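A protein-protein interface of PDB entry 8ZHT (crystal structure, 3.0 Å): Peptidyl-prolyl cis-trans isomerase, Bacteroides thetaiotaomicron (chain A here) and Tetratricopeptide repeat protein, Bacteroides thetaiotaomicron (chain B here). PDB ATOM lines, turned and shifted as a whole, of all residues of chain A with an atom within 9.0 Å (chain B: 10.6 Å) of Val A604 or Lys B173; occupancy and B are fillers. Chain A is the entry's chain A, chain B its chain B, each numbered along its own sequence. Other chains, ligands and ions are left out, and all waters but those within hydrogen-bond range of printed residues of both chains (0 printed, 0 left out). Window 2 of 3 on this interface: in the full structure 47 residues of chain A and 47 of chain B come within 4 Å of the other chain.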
ATOM      1  N   ASN A 174     -17.124 -14.813 -13.026  1.00  0.00           N
ATOM      2  CA  ASN A 174     -18.186 -14.758 -14.026  1.00  0.00           C
ATOM      3  C   ASN A 174     -19.197 -13.680 -13.630  1.00  0.00           C
ATOM      4  O   ASN A 174     -19.757 -13.712 -12.526  1.00  0.00           O
ATOM      5  CB  ASN A 174     -18.869 -16.115 -14.173  1.00  0.00           C
ATOM      6  CG  ASN A 174     -17.946 -17.176 -14.780  1.00  0.00           C
ATOM      7  OD1 ASN A 174     -17.301 -16.946 -15.782  1.00  0.00           O
ATOM      8  ND2 ASN A 174     -17.892 -18.335 -14.160  1.00  0.00           N
ATOM      9  N   TYR A 176     -22.571 -11.173 -14.926  1.00  0.00           N
ATOM     10  CA  TYR A 176     -23.740 -11.267 -15.780  1.00  0.00           C
ATOM     11  C   TYR A 176     -24.528  -9.971 -15.720  1.00  0.00           C
ATOM     12  O   TYR A 176     -24.519  -9.268 -14.707  1.00  0.00           O
ATOM     13  CB  TYR A 176     -24.641 -12.421 -15.342  1.00  0.00           C
ATOM     14  CG  TYR A 176     -23.929 -13.740 -15.172  1.00  0.00           C
ATOM     15  CD1 TYR A 176     -23.782 -14.619 -16.242  1.00  0.00           C
ATOM     16  CD2 TYR A 176     -23.414 -14.117 -13.935  1.00  0.00           C
ATOM     17  CE1 TYR A 176     -23.143 -15.832 -16.093  1.00  0.00           C
ATOM     18  CE2 TYR A 176     -22.768 -15.331 -13.775  1.00  0.00           C
ATOM     19  CZ  TYR A 176     -22.634 -16.177 -14.857  1.00  0.00           C
ATOM     20  OH  TYR A 176     -21.999 -17.366 -14.679  1.00  0.00           O
ATOM     21  N   LEU A 178     -28.488  -8.437 -16.455  1.00  0.00           N
ATOM     22  CA  LEU A 178     -29.831  -8.985 -16.559  1.00  0.00           C
ATOM     23  C   LEU A 178     -30.848  -7.886 -16.328  1.00  0.00           C
ATOM     24  O   LEU A 178     -30.644  -7.021 -15.476  1.00  0.00           O
ATOM     25  CB  LEU A 178     -30.062 -10.105 -15.532  1.00  0.00           C
ATOM     26  CG  LEU A 178     -29.062 -11.263 -15.455  1.00  0.00           C
ATOM     27  CD1 LEU A 178     -28.078 -11.003 -14.345  1.00  0.00           C
ATOM     28  CD2 LEU A 178     -29.795 -12.577 -15.220  1.00  0.00           C
ATOM     29  N   PHE A 582     -22.473 -14.987  -8.766  1.00  0.00           N
ATOM     30  CA  PHE A 582     -22.976 -15.937  -7.777  1.00  0.00           C
ATOM     31  C   PHE A 582     -22.467 -15.599  -6.378  1.00  0.00           C
ATOM     32  O   PHE A 582     -23.221 -15.680  -5.401  1.00  0.00           O
ATOM     33  CB  PHE A 582     -22.566 -17.348  -8.174  1.00  0.00           C
ATOM     34  CG  PHE A 582     -23.157 -18.429  -7.316  1.00  0.00           C
ATOM     35  CD1 PHE A 582     -24.449 -18.869  -7.525  1.00  0.00           C
ATOM     36  CD2 PHE A 582     -22.398 -19.038  -6.335  1.00  0.00           C
ATOM     37  CE1 PHE A 582     -24.993 -19.899  -6.744  1.00  0.00           C
ATOM     38  CE2 PHE A 582     -22.928 -20.062  -5.552  1.00  0.00           C
ATOM     39  CZ  PHE A 582     -24.229 -20.489  -5.757  1.00  0.00           C
ATOM     40  N   LEU A 597     -30.679 -14.708  -4.739  1.00  0.00           N
ATOM     41  CA  LEU A 597     -31.143 -15.642  -5.755  1.00  0.00           C
ATOM     42  C   LEU A 597     -30.933 -15.120  -7.178  1.00  0.00           C
ATOM     43  O   LEU A 597     -31.018 -15.908  -8.129  1.00  0.00           O
ATOM     44  CB  LEU A 597     -32.616 -15.983  -5.514  1.00  0.00           C
ATOM     45  CG  LEU A 597     -32.873 -16.962  -4.359  1.00  0.00           C
ATOM     46  CD1 LEU A 597     -34.318 -17.475  -4.341  1.00  0.00           C
ATOM     47  CD2 LEU A 597     -31.899 -18.143  -4.405  1.00  0.00           C
ATOM     48  N   VAL A 598     -30.667 -13.817  -7.351  1.00  0.00           N
ATOM     49  CA  VAL A 598     -30.390 -13.279  -8.685  1.00  0.00           C
ATOM     50  C   VAL A 598     -29.161 -13.954  -9.287  1.00  0.00           C
ATOM     51  O   VAL A 598     -29.170 -14.382 -10.450  1.00  0.00           O
ATOM     52  CB  VAL A 598     -30.209 -11.747  -8.627  1.00  0.00           C
ATOM     53  CG1 VAL A 598     -29.692 -11.216  -9.954  1.00  0.00           C
ATOM     54  CG2 VAL A 598     -31.508 -11.046  -8.231  1.00  0.00           C
ATOM     55  N   GLY A 599     -28.078 -14.044  -8.508  1.00  0.00           N
ATOM     56  CA  GLY A 599     -26.865 -14.686  -8.987  1.00  0.00           C
ATOM     57  C   GLY A 599     -26.996 -16.189  -9.150  1.00  0.00           C
ATOM     58  O   GLY A 599     -26.408 -16.766 -10.071  1.00  0.00           O
ATOM     59  N   ALA A 600     -27.769 -16.845  -8.282  1.00  0.00           N
ATOM     60  CA  ALA A 600     -28.035 -18.274  -8.457  1.00  0.00           C
ATOM     61  C   ALA A 600     -28.630 -18.537  -9.831  1.00  0.00           C
ATOM     62  O   ALA A 600     -28.126 -19.369 -10.598  1.00  0.00           O
ATOM     63  CB  ALA A 600     -28.983 -18.781  -7.362  1.00  0.00           C
ATOM     64  N   TYR A 601     -29.684 -17.793 -10.172  1.00  0.00           N
ATOM     65  CA  TYR A 601     -30.285 -17.913 -11.494  1.00  0.00           C
ATOM     66  C   TYR A 601     -29.282 -17.581 -12.586  1.00  0.00           C
ATOM     67  O   TYR A 601     -29.186 -18.294 -13.593  1.00  0.00           O
ATOM     68  CB  TYR A 601     -31.494 -16.990 -11.620  1.00  0.00           C
ATOM     69  CG  TYR A 601     -31.977 -16.984 -13.039  1.00  0.00           C
ATOM     70  CD1 TYR A 601     -32.700 -18.059 -13.531  1.00  0.00           C
ATOM     71  CD2 TYR A 601     -31.657 -15.941 -13.911  1.00  0.00           C
ATOM     72  CE1 TYR A 601     -33.125 -18.103 -14.847  1.00  0.00           C
ATOM     73  CE2 TYR A 601     -32.095 -15.962 -15.235  1.00  0.00           C
ATOM     74  CZ  TYR A 601     -32.822 -17.059 -15.693  1.00  0.00           C
ATOM     75  OH  TYR A 601     -33.267 -17.122 -16.989  1.00  0.00           O
ATOM     76  N   ALA A 602     -28.547 -16.475 -12.425  1.00  0.00           N
ATOM     77  CA  ALA A 602     -27.693 -16.033 -13.528  1.00  0.00           C
ATOM     78  C   ALA A 602     -26.594 -17.040 -13.828  1.00  0.00           C
ATOM     79  O   ALA A 602     -26.218 -17.215 -14.994  1.00  0.00           O
ATOM     80  CB  ALA A 602     -27.080 -14.654 -13.235  1.00  0.00           C
ATOM     81  N   SER A 603     -26.083 -17.725 -12.805  1.00  0.00           N
ATOM     82  CA  SER A 603     -24.976 -18.659 -13.012  1.00  0.00           C
ATOM     83  C   SER A 603     -25.338 -19.839 -13.909  1.00  0.00           C
ATOM     84  O   SER A 603     -24.428 -20.516 -14.396  1.00  0.00           O
ATOM     85  CB  SER A 603     -24.476 -19.195 -11.667  1.00  0.00           C
ATOM     86  OG  SER A 603     -25.488 -19.994 -11.046  1.00  0.00           O
ATOM     87  N   VAL A 604     -26.626 -20.126 -14.125  1.00  0.00           N
ATOM     88  CA  VAL A 604     -26.999 -21.259 -14.967  1.00  0.00           C
ATOM     89  C   VAL A 604     -28.015 -20.852 -16.037  1.00  0.00           C
ATOM     90  O   VAL A 604     -28.643 -21.705 -16.674  1.00  0.00           O
ATOM     91  CB  VAL A 604     -27.536 -22.420 -14.106  1.00  0.00           C
ATOM     92  CG1 VAL A 604     -26.461 -22.894 -13.098  1.00  0.00           C
ATOM     93  CG2 VAL A 604     -28.815 -22.015 -13.396  1.00  0.00           C
ATOM     94  N   ALA A 605     -28.168 -19.553 -16.271  1.00  0.00           N
ATOM     95  CA  ALA A 605     -29.210 -19.071 -17.171  1.00  0.00           C
ATOM     96  C   ALA A 605     -28.761 -19.066 -18.626  1.00  0.00           C
ATOM     97  O   ALA A 605     -27.572 -18.947 -18.938  1.00  0.00           O
ATOM     98  CB  ALA A 605     -29.648 -17.657 -16.795  1.00  0.00           C
ATOM     99  N   GLU A 606     -29.743 -19.174 -19.511  1.00  0.00           N
ATOM    100  CA  GLU A 606     -29.548 -19.066 -20.946  1.00  0.00           C
ATOM    101  C   GLU A 606     -29.718 -17.622 -21.362  1.00  0.00           C
ATOM    102  O   GLU A 606     -30.535 -16.883 -20.799  1.00  0.00           O
ATOM    103  CB  GLU A 606     -30.558 -19.931 -21.699  1.00  0.00           C
ATOM    104  CG  GLU A 606     -30.230 -21.420 -21.706  1.00  0.00           C
ATOM    105  CD  GLU A 606     -31.476 -22.271 -21.916  1.00  0.00           C
ATOM    106  OE1 GLU A 606     -32.055 -22.228 -23.032  1.00  0.00           O
ATOM    107  OE2 GLU A 606     -31.865 -22.997 -20.968  1.00  0.00           O
ATOM    108  N   MET A 607     -28.944 -17.228 -22.359  1.00  0.00           N
ATOM    109  CA  MET A 607     -28.971 -15.848 -22.815  1.00  0.00           C
ATOM    110  C   MET A 607     -30.290 -15.542 -23.513  1.00  0.00           C
ATOM    111  O   MET A 607     -30.763 -16.332 -24.332  1.00  0.00           O
ATOM    112  CB  MET A 607     -27.786 -15.577 -23.744  1.00  0.00           C
ATOM    113  CG  MET A 607     -27.757 -14.147 -24.190  1.00  0.00           C
ATOM    114  SD  MET A 607     -27.079 -13.093 -22.901  1.00  0.00           S
ATOM    115  CE  MET A 607     -25.498 -13.895 -22.617  1.00  0.00           C
ATOM    116  N   LYS A 609     -33.313 -15.580 -22.494  1.00  0.00           N
ATOM    117  CA  LYS A 609     -34.465 -16.375 -22.106  1.00  0.00           C
ATOM    118  C   LYS A 609     -35.048 -15.803 -20.812  1.00  0.00           C
ATOM    119  O   LYS A 609     -34.316 -15.584 -19.841  1.00  0.00           O
ATOM    120  CB  LYS A 609     -34.050 -17.844 -21.945  1.00  0.00           C
ATOM    121  CG  LYS A 609     -35.153 -18.793 -21.462  1.00  0.00           C
ATOM    122  CD  LYS A 609     -34.560 -20.144 -20.993  1.00  0.00           C
ATOM    123  CE  LYS A 609     -35.567 -21.285 -21.142  1.00  0.00           C
ATOM    124  NZ  LYS A 609     -36.956 -20.765 -21.320  1.00  0.00           N
ATOM    125  N   MET A 625     -31.357 -12.488 -18.876  1.00  0.00           N
ATOM    126  CA  MET A 625     -29.971 -12.090 -19.065  1.00  0.00           C
ATOM    127  C   MET A 625     -29.736 -11.594 -20.497  1.00  0.00           C
ATOM    128  O   MET A 625     -30.251 -12.161 -21.469  1.00  0.00           O
ATOM    129  CB  MET A 625     -29.047 -13.266 -18.736  1.00  0.00           C
ATOM    130  CG  MET A 625     -27.634 -13.144 -19.272  1.00  0.00           C
ATOM    131  SD  MET A 625     -26.565 -14.411 -18.515  1.00  0.00           S
ATOM    132  CE  MET A 625     -26.825 -15.683 -19.738  1.00  0.00           C
ATOM    133  N   LYS A 628     -22.839 -10.982 -20.554  1.00  0.00           N
ATOM    134  CA  LYS A 628     -21.957 -11.879 -19.810  1.00  0.00           C
ATOM    135  C   LYS A 628     -20.523 -11.442 -20.055  1.00  0.00           C
ATOM    136  O   LYS A 628     -20.199 -10.995 -21.150  1.00  0.00           O
ATOM    137  CB  LYS A 628     -22.070 -13.330 -20.296  1.00  0.00           C
ATOM    138  CG  LYS A 628     -22.957 -14.233 -19.524  1.00  0.00           C
ATOM    139  CD  LYS A 628     -22.998 -15.652 -20.152  1.00  0.00           C
ATOM    140  CE  LYS A 628     -21.875 -15.865 -21.149  1.00  0.00           C
ATOM    141  NZ  LYS A 628     -21.949 -17.205 -21.796  1.00  0.00           N
ATOM    142  N   VAL B 133     -22.799 -31.828  -7.361  1.00  0.00           N
ATOM    143  CA  VAL B 133     -23.247 -31.026  -8.499  1.00  0.00           C
ATOM    144  C   VAL B 133     -22.343 -31.259  -9.705  1.00  0.00           C
ATOM    145  O   VAL B 133     -22.827 -31.418 -10.832  1.00  0.00           O
ATOM    146  CB  VAL B 133     -23.312 -29.530  -8.131  1.00  0.00           C
ATOM    147  CG1 VAL B 133     -23.406 -28.657  -9.406  1.00  0.00           C
ATOM    148  CG2 VAL B 133     -24.489 -29.243  -7.203  1.00  0.00           C
ATOM    149  N   GLY B 136     -23.292 -34.072 -11.689  1.00  0.00           N
ATOM    150  CA  GLY B 136     -24.634 -34.087 -12.234  1.00  0.00           C
ATOM    151  C   GLY B 136     -25.684 -34.709 -11.341  1.00  0.00           C
ATOM    152  O   GLY B 136     -26.799 -34.974 -11.815  1.00  0.00           O
ATOM    153  N   TYR B 138     -27.953 -33.853  -9.058  1.00  0.00           N
ATOM    154  CA  TYR B 138     -28.530 -32.622  -8.533  1.00  0.00           C
ATOM    155  C   TYR B 138     -29.437 -32.884  -7.336  1.00  0.00           C
ATOM    156  O   TYR B 138     -29.384 -32.148  -6.339  1.00  0.00           O
ATOM    157  CB  TYR B 138     -29.258 -31.890  -9.658  1.00  0.00           C
ATOM    158  CG  TYR B 138     -28.333 -31.617 -10.820  1.00  0.00           C
ATOM    159  CD1 TYR B 138     -27.166 -30.887 -10.639  1.00  0.00           C
ATOM    160  CD2 TYR B 138     -28.600 -32.121 -12.088  1.00  0.00           C
ATOM    161  CE1 TYR B 138     -26.298 -30.640 -11.693  1.00  0.00           C
ATOM    162  CE2 TYR B 138     -27.735 -31.882 -13.154  1.00  0.00           C
ATOM    163  CZ  TYR B 138     -26.584 -31.140 -12.946  1.00  0.00           C
ATOM    164  OH  TYR B 138     -25.713 -30.888 -13.987  1.00  0.00           O
ATOM    165  N   ASP B 139     -30.253 -33.941  -7.383  1.00  0.00           N
ATOM    166  CA  ASP B 139     -31.117 -34.215  -6.235  1.00  0.00           C
ATOM    167  C   ASP B 139     -30.300 -34.530  -4.978  1.00  0.00           C
ATOM    168  O   ASP B 139     -30.663 -34.113  -3.875  1.00  0.00           O
ATOM    169  CB  ASP B 139     -32.083 -35.359  -6.556  1.00  0.00           C
ATOM    170  CG  ASP B 139     -33.036 -35.021  -7.702  1.00  0.00           C
ATOM    171  OD1 ASP B 139     -33.749 -33.998  -7.610  1.00  0.00           O
ATOM    172  OD2 ASP B 139     -33.066 -35.783  -8.699  1.00  0.00           O
ATOM    173  N   VAL B 142     -29.068 -31.264  -3.611  1.00  0.00           N
ATOM    174  CA  VAL B 142     -30.143 -30.547  -2.934  1.00  0.00           C
ATOM    175  C   VAL B 142     -30.371 -31.128  -1.542  1.00  0.00           C
ATOM    176  O   VAL B 142     -30.630 -30.388  -0.584  1.00  0.00           O
ATOM    177  CB  VAL B 142     -31.420 -30.571  -3.802  1.00  0.00           C
ATOM    178  CG1 VAL B 142     -32.649 -30.130  -3.013  1.00  0.00           C
ATOM    179  CG2 VAL B 142     -31.241 -29.657  -5.018  1.00  0.00           C
ATOM    180  N   LYS B 163     -29.005 -19.902  -2.191  1.00  0.00           N
ATOM    181  CA  LYS B 163     -28.540 -19.768  -3.564  1.00  0.00           C
ATOM    182  C   LYS B 163     -27.960 -21.072  -4.093  1.00  0.00           C
ATOM    183  O   LYS B 163     -28.014 -21.319  -5.301  1.00  0.00           O
ATOM    184  CB  LYS B 163     -27.528 -18.627  -3.677  1.00  0.00           C
ATOM    185  CG  LYS B 163     -26.152 -18.899  -3.106  1.00  0.00           C
ATOM    186  CD  LYS B 163     -25.267 -17.663  -3.302  1.00  0.00           C
ATOM    187  CE  LYS B 163     -24.013 -17.745  -2.452  1.00  0.00           C
ATOM    188  NZ  LYS B 163     -23.112 -16.580  -2.671  1.00  0.00           N
ATOM    189  N   TYR B 164     -27.426 -21.927  -3.218  1.00  0.00           N
ATOM    190  CA  TYR B 164     -26.902 -23.210  -3.679  1.00  0.00           C
ATOM    191  C   TYR B 164     -28.033 -24.186  -3.964  1.00  0.00           C
ATOM    192  O   TYR B 164     -27.973 -24.949  -4.936  1.00  0.00           O
ATOM    193  CB  TYR B 164     -25.941 -23.808  -2.639  1.00  0.00           C
ATOM    194  CG  TYR B 164     -24.622 -23.057  -2.500  1.00  0.00           C
ATOM    195  CD1 TYR B 164     -23.543 -23.354  -3.327  1.00  0.00           C
ATOM    196  CD2 TYR B 164     -24.468 -22.054  -1.548  1.00  0.00           C
ATOM    197  CE1 TYR B 164     -22.349 -22.669  -3.217  1.00  0.00           C
ATOM    198  CE2 TYR B 164     -23.268 -21.349  -1.430  1.00  0.00           C
ATOM    199  CZ  TYR B 164     -22.211 -21.668  -2.265  1.00  0.00           C
ATOM    200  OH  TYR B 164     -21.011 -20.997  -2.151  1.00  0.00           O
ATOM    201  N   ILE B 165     -29.061 -24.196  -3.114  1.00  0.00           N
ATOM    202  CA  ILE B 165     -30.217 -25.051  -3.368  1.00  0.00           C
ATOM    203  C   ILE B 165     -30.875 -24.650  -4.683  1.00  0.00           C
ATOM    204  O   ILE B 165     -31.157 -25.493  -5.544  1.00  0.00           O
ATOM    205  CB  ILE B 165     -31.213 -24.977  -2.196  1.00  0.00           C
ATOM    206  CG1 ILE B 165     -30.607 -25.580  -0.923  1.00  0.00           C
ATOM    207  CG2 ILE B 165     -32.527 -25.685  -2.573  1.00  0.00           C
ATOM    208  CD1 ILE B 165     -31.345 -25.157   0.371  1.00  0.00           C
ATOM    209  N   GLU B 166     -31.083 -23.342  -4.874  1.00  0.00           N
ATOM    210  CA  GLU B 166     -31.766 -22.870  -6.069  1.00  0.00           C
ATOM    211  C   GLU B 166     -30.973 -23.172  -7.326  1.00  0.00           C
ATOM    212  O   GLU B 166     -31.544 -23.585  -8.339  1.00  0.00           O
ATOM    213  CB  GLU B 166     -32.030 -21.373  -5.978  1.00  0.00           C
ATOM    214  CG  GLU B 166     -32.840 -20.890  -7.138  1.00  0.00           C
ATOM    215  CD  GLU B 166     -34.329 -21.033  -6.862  1.00  0.00           C
ATOM    216  OE1 GLU B 166     -34.691 -21.772  -5.902  1.00  0.00           O
ATOM    217  OE2 GLU B 166     -35.130 -20.394  -7.583  1.00  0.00           O
ATOM    218  N   GLN B 167     -29.653 -22.964  -7.291  1.00  0.00           N
ATOM    219  CA  GLN B 167     -28.844 -23.300  -8.461  1.00  0.00           C
ATOM    220  C   GLN B 167     -28.949 -24.787  -8.799  1.00  0.00           C
ATOM    221  O   GLN B 167     -29.072 -25.154  -9.974  1.00  0.00           O
ATOM    222  CB  GLN B 167     -27.386 -22.903  -8.238  1.00  0.00           C
ATOM    223  CG  GLN B 167     -26.409 -23.364  -9.316  1.00  0.00           C
ATOM    224  CD  GLN B 167     -24.945 -23.095  -8.908  1.00  0.00           C
ATOM    225  OE1 GLN B 167     -24.432 -23.707  -7.977  1.00  0.00           O
ATOM    226  NE2 GLN B 167     -24.293 -22.152  -9.589  1.00  0.00           N
ATOM    227  N   ALA B 168     -28.907 -25.663  -7.792  1.00  0.00           N
ATOM    228  CA  ALA B 168     -28.964 -27.092  -8.098  1.00  0.00           C
ATOM    229  C   ALA B 168     -30.342 -27.494  -8.624  1.00  0.00           C
ATOM    230  O   ALA B 168     -30.433 -28.301  -9.555  1.00  0.00           O
ATOM    231  CB  ALA B 168     -28.586 -27.928  -6.878  1.00  0.00           C
ATOM    232  N   LYS B 169     -31.421 -26.941  -8.047  1.00  0.00           N
ATOM    233  CA  LYS B 169     -32.767 -27.154  -8.595  1.00  0.00           C
ATOM    234  C   LYS B 169     -32.858 -26.704 -10.054  1.00  0.00           C
ATOM    235  O   LYS B 169     -33.394 -27.418 -10.900  1.00  0.00           O
ATOM    236  CB  LYS B 169     -33.815 -26.410  -7.755  1.00  0.00           C
ATOM    237  CG  LYS B 169     -34.444 -27.258  -6.662  1.00  0.00           C
ATOM    238  CD  LYS B 169     -35.350 -26.433  -5.737  1.00  0.00           C
ATOM    239  CE  LYS B 169     -35.762 -27.256  -4.499  1.00  0.00           C
ATOM    240  NZ  LYS B 169     -35.934 -26.444  -3.233  1.00  0.00           N
ATOM    241  N   LEU B 170     -32.339 -25.516 -10.364  1.00  0.00           N
ATOM    242  CA  LEU B 170     -32.408 -25.004 -11.729  1.00  0.00           C
ATOM    243  C   LEU B 170     -31.589 -25.829 -12.716  1.00  0.00           C
ATOM    244  O   LEU B 170     -31.858 -25.769 -13.919  1.00  0.00           O
ATOM    245  CB  LEU B 170     -31.932 -23.548 -11.778  1.00  0.00           C
ATOM    246  CG  LEU B 170     -32.843 -22.446 -11.219  1.00  0.00           C
ATOM    247  CD1 LEU B 170     -32.081 -21.103 -11.143  1.00  0.00           C
ATOM    248  CD2 LEU B 170     -34.132 -22.306 -12.037  1.00  0.00           C
ATOM    249  N   MET B 171     -30.593 -26.588 -12.260  1.00  0.00           N
ATOM    250  CA  MET B 171     -29.864 -27.402 -13.225  1.00  0.00           C
ATOM    251  C   MET B 171     -30.544 -28.734 -13.534  1.00  0.00           C
ATOM    252  O   MET B 171     -30.115 -29.413 -14.473  1.00  0.00           O
ATOM    253  CB  MET B 171     -28.422 -27.639 -12.759  1.00  0.00           C
ATOM    254  CG  MET B 171     -27.645 -26.364 -12.445  1.00  0.00           C
ATOM    255  SD  MET B 171     -26.048 -26.670 -11.618  1.00  0.00           S
ATOM    256  CE  MET B 171     -25.169 -27.608 -12.892  1.00  0.00           C
ATOM    257  N   LYS B 172     -31.582 -29.125 -12.786  1.00  0.00           N
ATOM    258  CA  LYS B 172     -32.357 -30.312 -13.156  1.00  0.00           C
ATOM    259  C   LYS B 172     -32.948 -30.152 -14.551  1.00  0.00           C
ATOM    260  O   LYS B 172     -32.821 -31.045 -15.402  1.00  0.00           O
ATOM    261  CB  LYS B 172     -33.460 -30.571 -12.127  1.00  0.00           C
ATOM    262  CG  LYS B 172     -32.977 -31.226 -10.843  1.00  0.00           C
ATOM    263  CD  LYS B 172     -34.119 -31.397  -9.847  1.00  0.00           C
ATOM    264  CE  LYS B 172     -35.010 -32.593 -10.211  1.00  0.00           C
ATOM    265  NZ  LYS B 172     -34.323 -33.640 -11.059  1.00  0.00           N
ATOM    266  N   LYS B 173     -33.590 -29.006 -14.800  1.00  0.00           N
ATOM    267  CA  LYS B 173     -33.989 -28.567 -16.143  1.00  0.00           C
ATOM    268  C   LYS B 173     -34.932 -29.571 -16.817  1.00  0.00           C
ATOM    269  O   LYS B 173     -35.371 -29.369 -17.954  1.00  0.00           O
ATOM    270  CB  LYS B 173     -32.743 -28.326 -17.023  1.00  0.00           C
ATOM    271  CG  LYS B 173     -32.239 -26.875 -17.057  1.00  0.00           C
ATOM    272  CD  LYS B 173     -30.736 -26.796 -17.362  1.00  0.00           C
ATOM    273  CE  LYS B 173     -30.107 -25.556 -16.718  1.00  0.00           C
ATOM    274  NZ  LYS B 173     -30.343 -24.283 -17.490  1.00  0.00           N
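NZ of Lys B173 sits at hydrogen-bond distance from O of Val A604, 3.2 Å away. The backbone carbonyl oxygen of Phe A582 is in hydrogen-bond range of the side-chain amino group of Lys B163, 2.9 Å away. The side-chain hydroxyl (OG) of Ser A603 is in hydrogen-bond range of the side-chain amide nitrogen (NE2) of Gln B167 (2.9 Å).
OH of Tyr A601 is in hydrogen-bond range of O of Lys A609, 3.4 Å away. The side-chain hydroxyl of Ser A603 lies within hydrogen-bond range of the backbone carbonyl oxygen of Ala A600 (2.7 Å). The backbone carbonyl oxygen (O) of Gly A599 lies close to the side-chain hydroxyl (OG) of Ser A603 (3.5 Å).
Tyr B164 touches Phe A582. Gln B167 touches Phe A582. CD2 of Leu A597 touches CA of Lys B163, 3.8 Å away. Leu A597 touches Glu B166. Ala A600 touches Lys B163 (CB to O, 3.4 Å). Leu B170 touches Tyr A601 (CD1 to CA, 3.7 Å). CG of Gln B167 touches CG1 of Val A604 (3.8 Å). Val A604 touches Leu B170 (CG2 to CB, 3.8 Å). CG1 of Val A604 touches CG of Met B171, at 3.7 Å.
Of chain B, only Gln B167 (3.8 Å), Leu B170 (3.8 Å), Met B171 (3.7 Å) and Lys B173 (3.2 Å) come within 4 Å of Val A604. Printed residues of chain A within 4 Å of Lys B173: Val A604 (3.2 Å). Ser A603 touches one residue of chain B. No residue of chain B comes within 4 Å of Ala A605. Met B171 touches just one residue of chain A: Val A604 (3.7 Å). Of the printed residues of chain B, Leu A597 touches Lys B163 (3.8 Å) and Glu B166 (3.6 Å). Printed residues of chain A within 4 Å of Tyr B164: Phe A582 (3.5 Å). Glu A606 touches none of the printed residues of chain B. Lys B172 touches none of the printed residues of chain A. The nearest printed residue of chain A that does not touch Lys B173 is Glu A606 (4.01 Å).
Printed residues of chain A that touch a printed residue of chain B: Phe A582, Leu A597, Ala A600, Tyr A601, Ser A603 and Val A604. Hydrophobic or aromatic side chains of chain A within 4 Å of the printed part of chain B: Phe A582, Leu A597, Ala A600, Tyr A601 and Val A604. Printed residues of chain B that touch a printed residue of chain A: Lys B163, Tyr B164, Glu B166, Gln B167, Leu B170, Met B171 and Lys B173. Among the printed residues, 12 pairs touch across the chains.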
